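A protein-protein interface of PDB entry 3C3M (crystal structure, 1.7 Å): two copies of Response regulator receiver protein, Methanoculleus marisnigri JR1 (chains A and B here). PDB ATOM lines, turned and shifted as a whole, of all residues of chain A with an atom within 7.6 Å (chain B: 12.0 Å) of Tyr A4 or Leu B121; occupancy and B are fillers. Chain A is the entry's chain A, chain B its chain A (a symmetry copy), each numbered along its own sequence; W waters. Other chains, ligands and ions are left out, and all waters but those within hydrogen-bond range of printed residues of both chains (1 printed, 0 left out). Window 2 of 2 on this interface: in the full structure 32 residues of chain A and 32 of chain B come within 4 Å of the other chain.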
ATOM      1  N   SER A   2       0.081  -4.692  -4.001  1.00  0.00           N
ATOM      2  CA  SER A   2      -0.079  -4.782  -5.485  1.00  0.00           C
ATOM      3  C   SER A   2      -1.177  -5.770  -5.844  1.00  0.00           C
ATOM      4  O   SER A   2      -1.536  -6.618  -5.030  1.00  0.00           O
ATOM      5  CB  SER A   2       1.238  -5.221  -6.136  1.00  0.00           C
ATOM      6  OG  SER A   2       1.641  -6.494  -5.655  1.00  0.00           O
ATOM      7  N   LEU A   3      -1.691  -5.664  -7.068  1.00  0.00           N
ATOM      8  CA  LEU A   3      -2.677  -6.618  -7.573  1.00  0.00           C
ATOM      9  C   LEU A   3      -2.210  -7.089  -8.942  1.00  0.00           C
ATOM     10  O   LEU A   3      -2.236  -6.311  -9.911  1.00  0.00           O
ATOM     11  CB  LEU A   3      -4.090  -6.014  -7.630  1.00  0.00           C
ATOM     12  CG  LEU A   3      -5.221  -6.890  -8.210  1.00  0.00           C
ATOM     13  CD1 LEU A   3      -5.453  -8.135  -7.347  1.00  0.00           C
ATOM     14  CD2 LEU A   3      -6.509  -6.098  -8.384  1.00  0.00           C
ATOM     15  N   TYR A   4      -1.813  -8.373  -8.982  1.00  0.00           N
ATOM     16  CA  TYR A   4      -1.278  -9.101 -10.152  1.00  0.00           C
ATOM     17  C   TYR A   4       0.214  -8.843 -10.350  1.00  0.00           C
ATOM     18  O   TYR A   4       0.669  -7.684 -10.373  1.00  0.00           O
ATOM     19  CB  TYR A   4      -2.033  -8.837 -11.461  1.00  0.00           C
ATOM     20  CG  TYR A   4      -3.557  -8.873 -11.389  1.00  0.00           C
ATOM     21  CD1 TYR A   4      -4.233  -9.870 -10.661  1.00  0.00           C
ATOM     22  CD2 TYR A   4      -4.313  -7.904 -12.044  1.00  0.00           C
ATOM     23  CE1 TYR A   4      -5.619  -9.892 -10.593  1.00  0.00           C
ATOM     24  CE2 TYR A   4      -5.710  -7.925 -11.997  1.00  0.00           C
ATOM     25  CZ  TYR A   4      -6.352  -8.914 -11.260  1.00  0.00           C
ATOM     26  OH  TYR A   4      -7.723  -8.924 -11.216  1.00  0.00           O
ATOM     27  N   THR A   5       0.965  -9.932 -10.496  1.00  0.00           N
ATOM     28  CA  THR A   5       2.400  -9.872 -10.757  1.00  0.00           C
ATOM     29  C   THR A   5       2.636 -10.149 -12.244  1.00  0.00           C
ATOM     30  O   THR A   5       2.190 -11.174 -12.773  1.00  0.00           O
ATOM     31  CB  THR A   5       3.152 -10.872  -9.863  1.00  0.00           C
ATOM     32  OG1 THR A   5       3.014 -10.463  -8.497  1.00  0.00           O
ATOM     33  CG2 THR A   5       4.617 -10.938 -10.196  1.00  0.00           C
ATOM     34  N   ILE A   6       3.349  -9.230 -12.897  1.00  0.00           N
ATOM     35  CA  ILE A   6       3.504  -9.238 -14.352  1.00  0.00           C
ATOM     36  C   ILE A   6       4.989  -9.315 -14.677  1.00  0.00           C
ATOM     37  O   ILE A   6       5.756  -8.433 -14.295  1.00  0.00           O
ATOM     38  CB  ILE A   6       2.932  -7.952 -15.007  1.00  0.00           C
ATOM     39  CG1 ILE A   6       1.521  -7.603 -14.487  1.00  0.00           C
ATOM     40  CG2 ILE A   6       2.923  -8.107 -16.543  1.00  0.00           C
ATOM     41  CD1 ILE A   6       0.462  -8.641 -14.855  1.00  0.00           C
ATOM     42  N   LEU A   7       5.409 -10.378 -15.365  1.00  0.00           N
ATOM     43  CA  LEU A   7       6.805 -10.487 -15.799  1.00  0.00           C
ATOM     44  C   LEU A   7       6.945  -9.872 -17.176  1.00  0.00           C
ATOM     45  O   LEU A   7       6.288 -10.298 -18.131  1.00  0.00           O
ATOM     46  CB  LEU A   7       7.259 -11.955 -15.855  1.00  0.00           C
ATOM     47  CG  LEU A   7       8.663 -12.193 -16.435  1.00  0.00           C
ATOM     48  CD1 LEU A   7       9.805 -11.482 -15.683  1.00  0.00           C
ATOM     49  CD2 LEU A   7       8.920 -13.713 -16.532  1.00  0.00           C
ATOM     50  N   LEU A  23       2.938  -0.209 -15.556  1.00  0.00           N
ATOM     51  CA  LEU A  23       2.380  -1.218 -14.641  1.00  0.00           C
ATOM     52  C   LEU A  23       2.344  -0.710 -13.210  1.00  0.00           C
ATOM     53  O   LEU A  23       1.334  -0.854 -12.528  1.00  0.00           O
ATOM     54  CB  LEU A  23       3.180  -2.518 -14.744  1.00  0.00           C
ATOM     55  CG  LEU A  23       2.989  -3.192 -16.099  1.00  0.00           C
ATOM     56  CD1 LEU A  23       4.068  -4.269 -16.318  1.00  0.00           C
ATOM     57  CD2 LEU A  23       1.578  -3.763 -16.257  1.00  0.00           C
ATOM     58  N   GLY A  26      -0.499   1.534 -11.997  1.00  0.00           N
ATOM     59  CA  GLY A  26      -1.752   0.812 -11.847  1.00  0.00           C
ATOM     60  C   GLY A  26      -1.718  -0.194 -10.712  1.00  0.00           C
ATOM     61  O   GLY A  26      -2.671  -0.945 -10.534  1.00  0.00           O
ATOM     62  N   GLY A  27      -0.638  -0.205  -9.938  1.00  0.00           N
ATOM     63  CA  GLY A  27      -0.504  -1.175  -8.843  1.00  0.00           C
ATOM     64  C   GLY A  27      -0.328  -2.630  -9.244  1.00  0.00           C
ATOM     65  O   GLY A  27      -0.549  -3.520  -8.445  1.00  0.00           O
ATOM     66  N   TYR A  28       0.062  -2.880 -10.488  1.00  0.00           N
ATOM     67  CA  TYR A  28       0.536  -4.208 -10.887  1.00  0.00           C
ATOM     68  C   TYR A  28       1.957  -4.323 -10.339  1.00  0.00           C
ATOM     69  O   TYR A  28       2.647  -3.309 -10.179  1.00  0.00           O
ATOM     70  CB  TYR A  28       0.580  -4.306 -12.421  1.00  0.00           C
ATOM     71  CG  TYR A  28      -0.751  -4.082 -13.143  1.00  0.00           C
ATOM     72  CD1 TYR A  28      -1.667  -5.127 -13.314  1.00  0.00           C
ATOM     73  CD2 TYR A  28      -1.088  -2.824 -13.659  1.00  0.00           C
ATOM     74  CE1 TYR A  28      -2.891  -4.917 -13.976  1.00  0.00           C
ATOM     75  CE2 TYR A  28      -2.295  -2.605 -14.324  1.00  0.00           C
ATOM     76  CZ  TYR A  28      -3.196  -3.652 -14.474  1.00  0.00           C
ATOM     77  OH  TYR A  28      -4.389  -3.413 -15.129  1.00  0.00           O
ATOM     78  N   ARG A  29       2.405  -5.538 -10.028  1.00  0.00           N
ATOM     79  CA  ARG A  29       3.781  -5.718  -9.570  1.00  0.00           C
ATOM     80  C   ARG A  29       4.646  -6.215 -10.730  1.00  0.00           C
ATOM     81  O   ARG A  29       4.520  -7.368 -11.162  1.00  0.00           O
ATOM     82  CB  ARG A  29       3.850  -6.729  -8.425  1.00  0.00           C
ATOM     83  CG  ARG A  29       5.246  -6.970  -7.935  1.00  0.00           C
ATOM     84  CD  ARG A  29       5.283  -7.924  -6.760  1.00  0.00           C
ATOM     85  NE  ARG A  29       6.665  -8.139  -6.338  1.00  0.00           N
ATOM     86  CZ  ARG A  29       7.325  -9.292  -6.432  1.00  0.00           C
ATOM     87  NH1 ARG A  29       6.733 -10.378  -6.922  1.00  0.00           N
ATOM     88  NH2 ARG A  29       8.588  -9.361  -6.026  1.00  0.00           N
ATOM     89  N   PRO A  30       5.518  -5.350 -11.260  1.00  0.00           N
ATOM     90  CA  PRO A  30       6.329  -5.830 -12.374  1.00  0.00           C
ATOM     91  C   PRO A  30       7.624  -6.508 -11.945  1.00  0.00           C
ATOM     92  O   PRO A  30       8.296  -6.058 -11.009  1.00  0.00           O
ATOM     93  CB  PRO A  30       6.649  -4.556 -13.161  1.00  0.00           C
ATOM     94  CG  PRO A  30       6.374  -3.410 -12.217  1.00  0.00           C
ATOM     95  CD  PRO A  30       5.801  -3.937 -10.934  1.00  0.00           C
ATOM     96  N   PRO A  48       5.007 -15.480 -11.959  1.00  0.00           N
ATOM     97  CA  PRO A  48       4.071 -14.376 -12.072  1.00  0.00           C
ATOM     98  C   PRO A  48       2.662 -14.847 -12.435  1.00  0.00           C
ATOM     99  O   PRO A  48       2.447 -16.038 -12.723  1.00  0.00           O
ATOM    100  CB  PRO A  48       4.679 -13.554 -13.218  1.00  0.00           C
ATOM    101  CG  PRO A  48       5.195 -14.634 -14.178  1.00  0.00           C
ATOM    102  CD  PRO A  48       5.701 -15.742 -13.240  1.00  0.00           C
ATOM    103  N   ASP A  49       1.711 -13.922 -12.431  1.00  0.00           N
ATOM    104  CA  ASP A  49       0.362 -14.206 -12.857  1.00  0.00           C
ATOM    105  C   ASP A  49       0.225 -14.120 -14.368  1.00  0.00           C
ATOM    106  O   ASP A  49      -0.729 -14.647 -14.932  1.00  0.00           O
ATOM    107  CB  ASP A  49      -0.621 -13.235 -12.204  1.00  0.00           C
ATOM    108  CG  ASP A  49      -0.618 -13.356 -10.711  1.00  0.00           C
ATOM    109  OD1 ASP A  49      -0.844 -14.471 -10.185  1.00  0.00           O
ATOM    110  OD2 ASP A  49      -0.348 -12.342 -10.058  1.00  0.00           O
ATOM    111  N   LEU A  50       1.159 -13.428 -15.014  1.00  0.00           N
ATOM    112  CA  LEU A  50       1.088 -13.208 -16.453  1.00  0.00           C
ATOM    113  C   LEU A  50       2.460 -12.799 -16.982  1.00  0.00           C
ATOM    114  O   LEU A  50       3.221 -12.143 -16.279  1.00  0.00           O
ATOM    115  CB  LEU A  50       0.028 -12.136 -16.775  1.00  0.00           C
ATOM    116  CG  LEU A  50      -0.285 -11.804 -18.239  1.00  0.00           C
ATOM    117  CD1 LEU A  50      -1.755 -11.485 -18.486  1.00  0.00           C
ATOM    118  CD2 LEU A  50       0.579 -10.640 -18.700  1.00  0.00           C
ATOM    119  N   VAL A  51       2.751 -13.176 -18.229  1.00  0.00           N
ATOM    120  CA  VAL A  51       4.023 -12.809 -18.869  1.00  0.00           C
ATOM    121  C   VAL A  51       3.775 -11.926 -20.094  1.00  0.00           C
ATOM    122  O   VAL A  51       2.880 -12.216 -20.898  1.00  0.00           O
ATOM    123  CB  VAL A  51       4.818 -14.067 -19.346  1.00  0.00           C
ATOM    124  CG1 VAL A  51       6.161 -13.657 -19.963  1.00  0.00           C
ATOM    125  CG2 VAL A  51       5.053 -15.012 -18.222  1.00  0.00           C
ATOM    126  N   PRO A  79      -0.551 -17.415 -18.267  1.00  0.00           N
ATOM    127  CA  PRO A  79      -0.950 -16.704 -19.483  1.00  0.00           C
ATOM    128  C   PRO A  79       0.170 -15.819 -20.040  1.00  0.00           C
ATOM    129  O   PRO A  79       0.957 -15.247 -19.275  1.00  0.00           O
ATOM    130  CB  PRO A  79      -2.150 -15.855 -19.050  1.00  0.00           C
ATOM    131  CG  PRO A  79      -2.095 -15.806 -17.568  1.00  0.00           C
ATOM    132  CD  PRO A  79      -1.350 -17.009 -17.089  1.00  0.00           C
ATOM    133  N   GLN B 112      -4.062  -0.358 -24.294  1.00  0.00           N
ATOM    134  CA  GLN B 112      -4.092  -1.735 -24.791  1.00  0.00           C
ATOM    135  C   GLN B 112      -3.533  -2.696 -23.752  1.00  0.00           C
ATOM    136  O   GLN B 112      -4.066  -3.795 -23.572  1.00  0.00           O
ATOM    137  CB  GLN B 112      -3.346  -1.885 -26.123  1.00  0.00           C
ATOM    138  CG  GLN B 112      -4.094  -1.321 -27.328  1.00  0.00           C
ATOM    139  CD  GLN B 112      -4.057   0.206 -27.400  1.00  0.00           C
ATOM    140  OE1 GLN B 112      -5.059   0.862 -27.149  1.00  0.00           O
ATOM    141  NE2 GLN B 112      -2.898   0.767 -27.745  1.00  0.00           N
ATOM    142  N   LEU B 113      -2.483  -2.259 -23.055  1.00  0.00           N
ATOM    143  CA  LEU B 113      -1.845  -3.065 -22.019  1.00  0.00           C
ATOM    144  C   LEU B 113      -2.817  -3.394 -20.870  1.00  0.00           C
ATOM    145  O   LEU B 113      -2.980  -4.570 -20.510  1.00  0.00           O
ATOM    146  CB  LEU B 113      -0.610  -2.347 -21.478  1.00  0.00           C
ATOM    147  CG  LEU B 113       0.091  -3.005 -20.295  1.00  0.00           C
ATOM    148  CD1 LEU B 113       0.786  -4.303 -20.703  1.00  0.00           C
ATOM    149  CD2 LEU B 113       1.073  -2.033 -19.688  1.00  0.00           C
ATOM    150  N   TYR B 114      -3.469  -2.369 -20.311  1.00  0.00           N
ATOM    151  CA  TYR B 114      -4.348  -2.607 -19.162  1.00  0.00           C
ATOM    152  C   TYR B 114      -5.553  -3.457 -19.582  1.00  0.00           C
ATOM    153  O   TYR B 114      -5.929  -4.387 -18.878  1.00  0.00           O
ATOM    154  CB  TYR B 114      -4.824  -1.276 -18.560  1.00  0.00           C
ATOM    155  CG  TYR B 114      -3.858  -0.580 -17.613  1.00  0.00           C
ATOM    156  CD1 TYR B 114      -2.454  -0.608 -17.807  1.00  0.00           C
ATOM    157  CD2 TYR B 114      -4.359   0.145 -16.519  1.00  0.00           C
ATOM    158  CE1 TYR B 114      -1.589   0.072 -16.914  1.00  0.00           C
ATOM    159  CE2 TYR B 114      -3.533   0.824 -15.665  1.00  0.00           C
ATOM    160  CZ  TYR B 114      -2.147   0.780 -15.847  1.00  0.00           C
ATOM    161  OH  TYR B 114      -1.359   1.462 -14.979  1.00  0.00           O
ATOM    162  N   GLU B 115      -6.118  -3.143 -20.742  1.00  0.00           N
ATOM    163  CA  GLU B 115      -7.285  -3.858 -21.268  1.00  0.00           C
ATOM    164  C   GLU B 115      -6.976  -5.342 -21.433  1.00  0.00           C
ATOM    165  O   GLU B 115      -7.752  -6.189 -20.997  1.00  0.00           O
ATOM    166  CB  GLU B 115      -7.689  -3.270 -22.621  1.00  0.00           C
ATOM    167  CG  GLU B 115      -9.039  -3.727 -23.147  1.00  0.00           C
ATOM    168  CD  GLU B 115      -9.312  -3.236 -24.574  1.00  0.00           C
ATOM    169  OE1 GLU B 115      -8.683  -2.242 -25.012  1.00  0.00           O
ATOM    170  OE2 GLU B 115     -10.159  -3.855 -25.259  1.00  0.00           O
ATOM    171  N   ALA B 116      -5.833  -5.646 -22.044  1.00  0.00           N
ATOM    172  CA  ALA B 116      -5.424  -7.045 -22.259  1.00  0.00           C
ATOM    173  C   ALA B 116      -5.159  -7.792 -20.948  1.00  0.00           C
ATOM    174  O   ALA B 116      -5.561  -8.956 -20.800  1.00  0.00           O
ATOM    175  CB  ALA B 116      -4.200  -7.113 -23.174  1.00  0.00           C
ATOM    176  N   ILE B 117      -4.500  -7.140 -19.989  1.00  0.00           N
ATOM    177  CA  ILE B 117      -4.200  -7.787 -18.699  1.00  0.00           C
ATOM    178  C   ILE B 117      -5.497  -7.993 -17.921  1.00  0.00           C
ATOM    179  O   ILE B 117      -5.732  -9.078 -17.393  1.00  0.00           O
ATOM    180  CB  ILE B 117      -3.178  -6.998 -17.840  1.00  0.00           C
ATOM    181  CG1 ILE B 117      -1.808  -6.980 -18.519  1.00  0.00           C
ATOM    182  CG2 ILE B 117      -3.052  -7.586 -16.415  1.00  0.00           C
ATOM    183  CD1 ILE B 117      -0.804  -6.097 -17.779  1.00  0.00           C
ATOM    184  N   GLU B 118      -6.331  -6.958 -17.859  1.00  0.00           N
ATOM    185  CA  GLU B 118      -7.617  -7.066 -17.144  1.00  0.00           C
ATOM    186  C   GLU B 118      -8.491  -8.164 -17.744  1.00  0.00           C
ATOM    187  O   GLU B 118      -9.054  -8.968 -17.001  1.00  0.00           O
ATOM    188  CB  GLU B 118      -8.356  -5.721 -17.088  1.00  0.00           C
ATOM    189  CG  GLU B 118      -7.656  -4.672 -16.192  1.00  0.00           C
ATOM    190  CD  GLU B 118      -7.509  -5.101 -14.727  1.00  0.00           C
ATOM    191  OE1 GLU B 118      -8.485  -5.586 -14.114  1.00  0.00           O
ATOM    192  OE2 GLU B 118      -6.403  -4.940 -14.172  1.00  0.00           O
ATOM    193  N   HIS B 119      -8.550  -8.235 -19.073  1.00  0.00           N
ATOM    194  CA  HIS B 119      -9.357  -9.257 -19.762  1.00  0.00           C
ATOM    195  C   HIS B 119      -8.938 -10.668 -19.360  1.00  0.00           C
ATOM    196  O   HIS B 119      -9.779 -11.568 -19.233  1.00  0.00           O
ATOM    197  CB  HIS B 119      -9.283  -9.103 -21.287  1.00  0.00           C
ATOM    198  CG  HIS B 119     -10.278  -9.947 -22.026  1.00  0.00           C
ATOM    199  ND1 HIS B 119      -9.923 -11.076 -22.731  1.00  0.00           N
ATOM    200  CD2 HIS B 119     -11.623  -9.838 -22.146  1.00  0.00           C
ATOM    201  CE1 HIS B 119     -11.004 -11.619 -23.263  1.00  0.00           C
ATOM    202  NE2 HIS B 119     -12.049 -10.887 -22.923  1.00  0.00           N
ATOM    203  N   VAL B 120      -7.635 -10.862 -19.146  1.00  0.00           N
ATOM    204  CA  VAL B 120      -7.107 -12.167 -18.746  1.00  0.00           C
ATOM    205  C   VAL B 120      -7.335 -12.441 -17.263  1.00  0.00           C
ATOM    206  O   VAL B 120      -7.783 -13.525 -16.893  1.00  0.00           O
ATOM    207  CB  VAL B 120      -5.575 -12.311 -19.056  1.00  0.00           C
ATOM    208  CG1 VAL B 120      -5.032 -13.620 -18.504  1.00  0.00           C
ATOM    209  CG2 VAL B 120      -5.320 -12.228 -20.538  1.00  0.00           C
ATOM    210  N   LEU B 121      -7.047 -11.460 -16.415  1.00  0.00           N
ATOM    211  CA  LEU B 121      -6.896 -11.739 -14.994  1.00  0.00           C
ATOM    212  C   LEU B 121      -8.071 -11.336 -14.104  1.00  0.00           C
ATOM    213  O   LEU B 121      -8.213 -11.890 -13.007  1.00  0.00           O
ATOM    214  CB  LEU B 121      -5.602 -11.135 -14.443  1.00  0.00           C
ATOM    215  CG  LEU B 121      -4.257 -11.627 -15.010  1.00  0.00           C
ATOM    216  CD1 LEU B 121      -3.137 -10.833 -14.397  1.00  0.00           C
ATOM    217  CD2 LEU B 121      -4.006 -13.120 -14.802  1.00  0.00           C
ATOM    218  N   ALA B 122      -8.871 -10.367 -14.542  1.00  0.00           N
ATOM    219  CA  ALA B 122     -10.017  -9.915 -13.718  1.00  0.00           C
ATOM    220  C   ALA B 122     -11.129 -10.970 -13.752  1.00  0.00           C
ATOM    221  O   ALA B 122     -11.254 -11.714 -14.734  1.00  0.00           O
ATOM    222  CB  ALA B 122     -10.548  -8.563 -14.191  1.00  0.00           C
ATOM    223  N   ARG B 123     -11.913 -11.041 -12.674  1.00  0.00           N
ATOM    224  CA  ARG B 123     -13.074 -11.935 -12.607  1.00  0.00           C
ATOM    225  C   ARG B 123     -14.175 -11.423 -13.527  1.00  0.00           C
ATOM    226  O   ARG B 123     -14.704 -10.329 -13.322  1.00  0.00           O
ATOM    227  CB  ARG B 123     -13.604 -12.065 -11.170  1.00  0.00           C
ATOM    228  CG  ARG B 123     -13.057 -13.251 -10.373  1.00  0.00           C
ATOM    229  CD  ARG B 123     -11.627 -13.014  -9.893  1.00  0.00           C
ATOM    230  NE  ARG B 123     -11.234 -13.907  -8.802  1.00  0.00           N
ATOM    231  CZ  ARG B 123     -11.071 -13.533  -7.534  1.00  0.00           C
ATOM    232  NH1 ARG B 123     -11.259 -12.270  -7.166  1.00  0.00           N
ATOM    233  NH2 ARG B 123     -10.709 -14.428  -6.624  1.00  0.00           N
ATOM    234  N   ARG B 124     -14.489 -12.220 -14.546  1.00  0.00           N
ATOM    235  CA  ARG B 124     -15.513 -11.896 -15.547  1.00  0.00           C
ATOM    236  C   ARG B 124     -16.919 -12.232 -15.057  1.00  0.00           C
ATOM    237  O   ARG B 124     -17.840 -11.427 -15.198  1.00  0.00           O
ATOM    238  CB  ARG B 124     -15.226 -12.607 -16.886  1.00  0.00           C
ATOM    239  CG  ARG B 124     -14.283 -13.828 -16.804  1.00  0.00           C
ATOM    240  CD  ARG B 124     -14.951 -15.086 -16.228  1.00  0.00           C
ATOM    241  NE  ARG B 124     -14.077 -15.762 -15.264  1.00  0.00           N
ATOM    242  CZ  ARG B 124     -14.240 -15.735 -13.940  1.00  0.00           C
ATOM    243  NH1 ARG B 124     -13.386 -16.378 -13.151  1.00  0.00           N
ATOM    244  NH2 ARG B 124     -15.257 -15.077 -13.396  1.00  0.00           N
HETATM  245  O   HOH W   1      -8.768  -6.435 -11.588  1.00  0.00           O
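The side-chain hydroxyl of Tyr A4 lies within hydrogen-bond range of the backbone carbonyl oxygen of Leu B121, at 3.5 Å.
N of Gly A26 lies within hydrogen-bond range of OH of Tyr B114 (3.1 Å).
OE2 of Glu B118 lies within hydrogen-bond range of OH of Tyr A28 (2.7 Å).
The backbone carbonyl oxygen (O) of Tyr A4 lies within hydrogen-bond range of the backbone NH (N) of Arg A29 (2.8 Å).
OD2 of Asp A49 lies within hydrogen-bond range of N of Thr A5 (2.8 Å).
The backbone carbonyl oxygen (O) of Thr A5 sits at hydrogen-bond distance from the backbone NH (N) of Leu A50.
The backbone NH (N) of Leu A7 is in hydrogen-bond range of the backbone carbonyl oxygen (O) of Leu A50 (3.0 Å).
The backbone carbonyl oxygen (O) of Leu A23 sits at hydrogen-bond distance from the backbone NH (N) of Tyr A28.
The backbone NH (N) of Val A51 sits at hydrogen-bond distance from the backbone carbonyl oxygen (O) of Pro A79, at 2.9 Å.
Tyr A4 touches Glu B118.
Tyr A4 touches Ala B122.
Ile B117 touches Ile A6.
CD2 of Leu A23 touches CD2 of Leu B113, at 3.9 Å.
Ile B117 touches Leu A23.
CE2 of Tyr A28 touches CZ of Tyr B114 (3.7 Å).
CE1 of Tyr A28 touches CG2 of Ile B117, 3.6 Å away.
CD2 of Leu B121 touches O of Asp A49, 3.6 Å away.
CG1 of Val B120 touches CD1 of Leu A50, at 3.9 Å.
Val B120 touches Pro A79 (CG1 to CB, 3.7 Å).
Of the printed residues of chain B, Tyr A4 touches Glu B118 (3.8 Å), Leu B121 (3.5 Å) and Ala B122 (3.5 Å).
No residue of chain B comes within 4 Å of Thr A5.
Of the printed residues of chain B, Ile A6 touches Ile B117.
Leu A7 touches none of the printed residues of chain B.
Tyr A28 touches just these residues of chain B: Tyr B114, Ile B117 and Glu B118.
No residue of chain B comes within 4 Å of Pro A30.
Leu A50 touches just one residue of chain B: Val B120 (3.9 Å).
Printed residues of chain B within 4 Å of Pro A79: Val B120 (3.7 Å).
Printed residues of chain A within 4 Å of Leu B113: Leu A23 (3.9 Å).
Of the printed residues of chain A, Glu B118 touches Tyr A4 and Tyr A28.
Of the printed residues of chain A, Val B120 touches Leu A50 (3.9 Å) and Pro A79 (3.7 Å).
Of chain A, only Tyr A4 and Asp A49 come within 4 Å of Leu B121.
Printed residues of chain A within 4 Å of Ala B122: Tyr A4.
The nearest printed residue of chain A that does not touch Ile B117 is Leu A50 (4.4 Å).
Hydrophobic or aromatic side chains of chain A that line the printed part of chain B: Tyr A4, Ile A6, Leu A23, Tyr A28, Leu A50 and Pro A79.
Among the printed residues, no Asp or Glu carboxylate lies within 4 Å of a Lys or Arg side-chain nitrogen of the other chain.
No position is printed for both chains.
Of the 13 pairs that touch across the chains among the printed residues, none has its exchanged pair printed and touching as well.
Water W1 lies within hydrogen-bond range of OE1 of Glu B118 (2.7 Å) and OH of Tyr A4 (2.7 Å).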
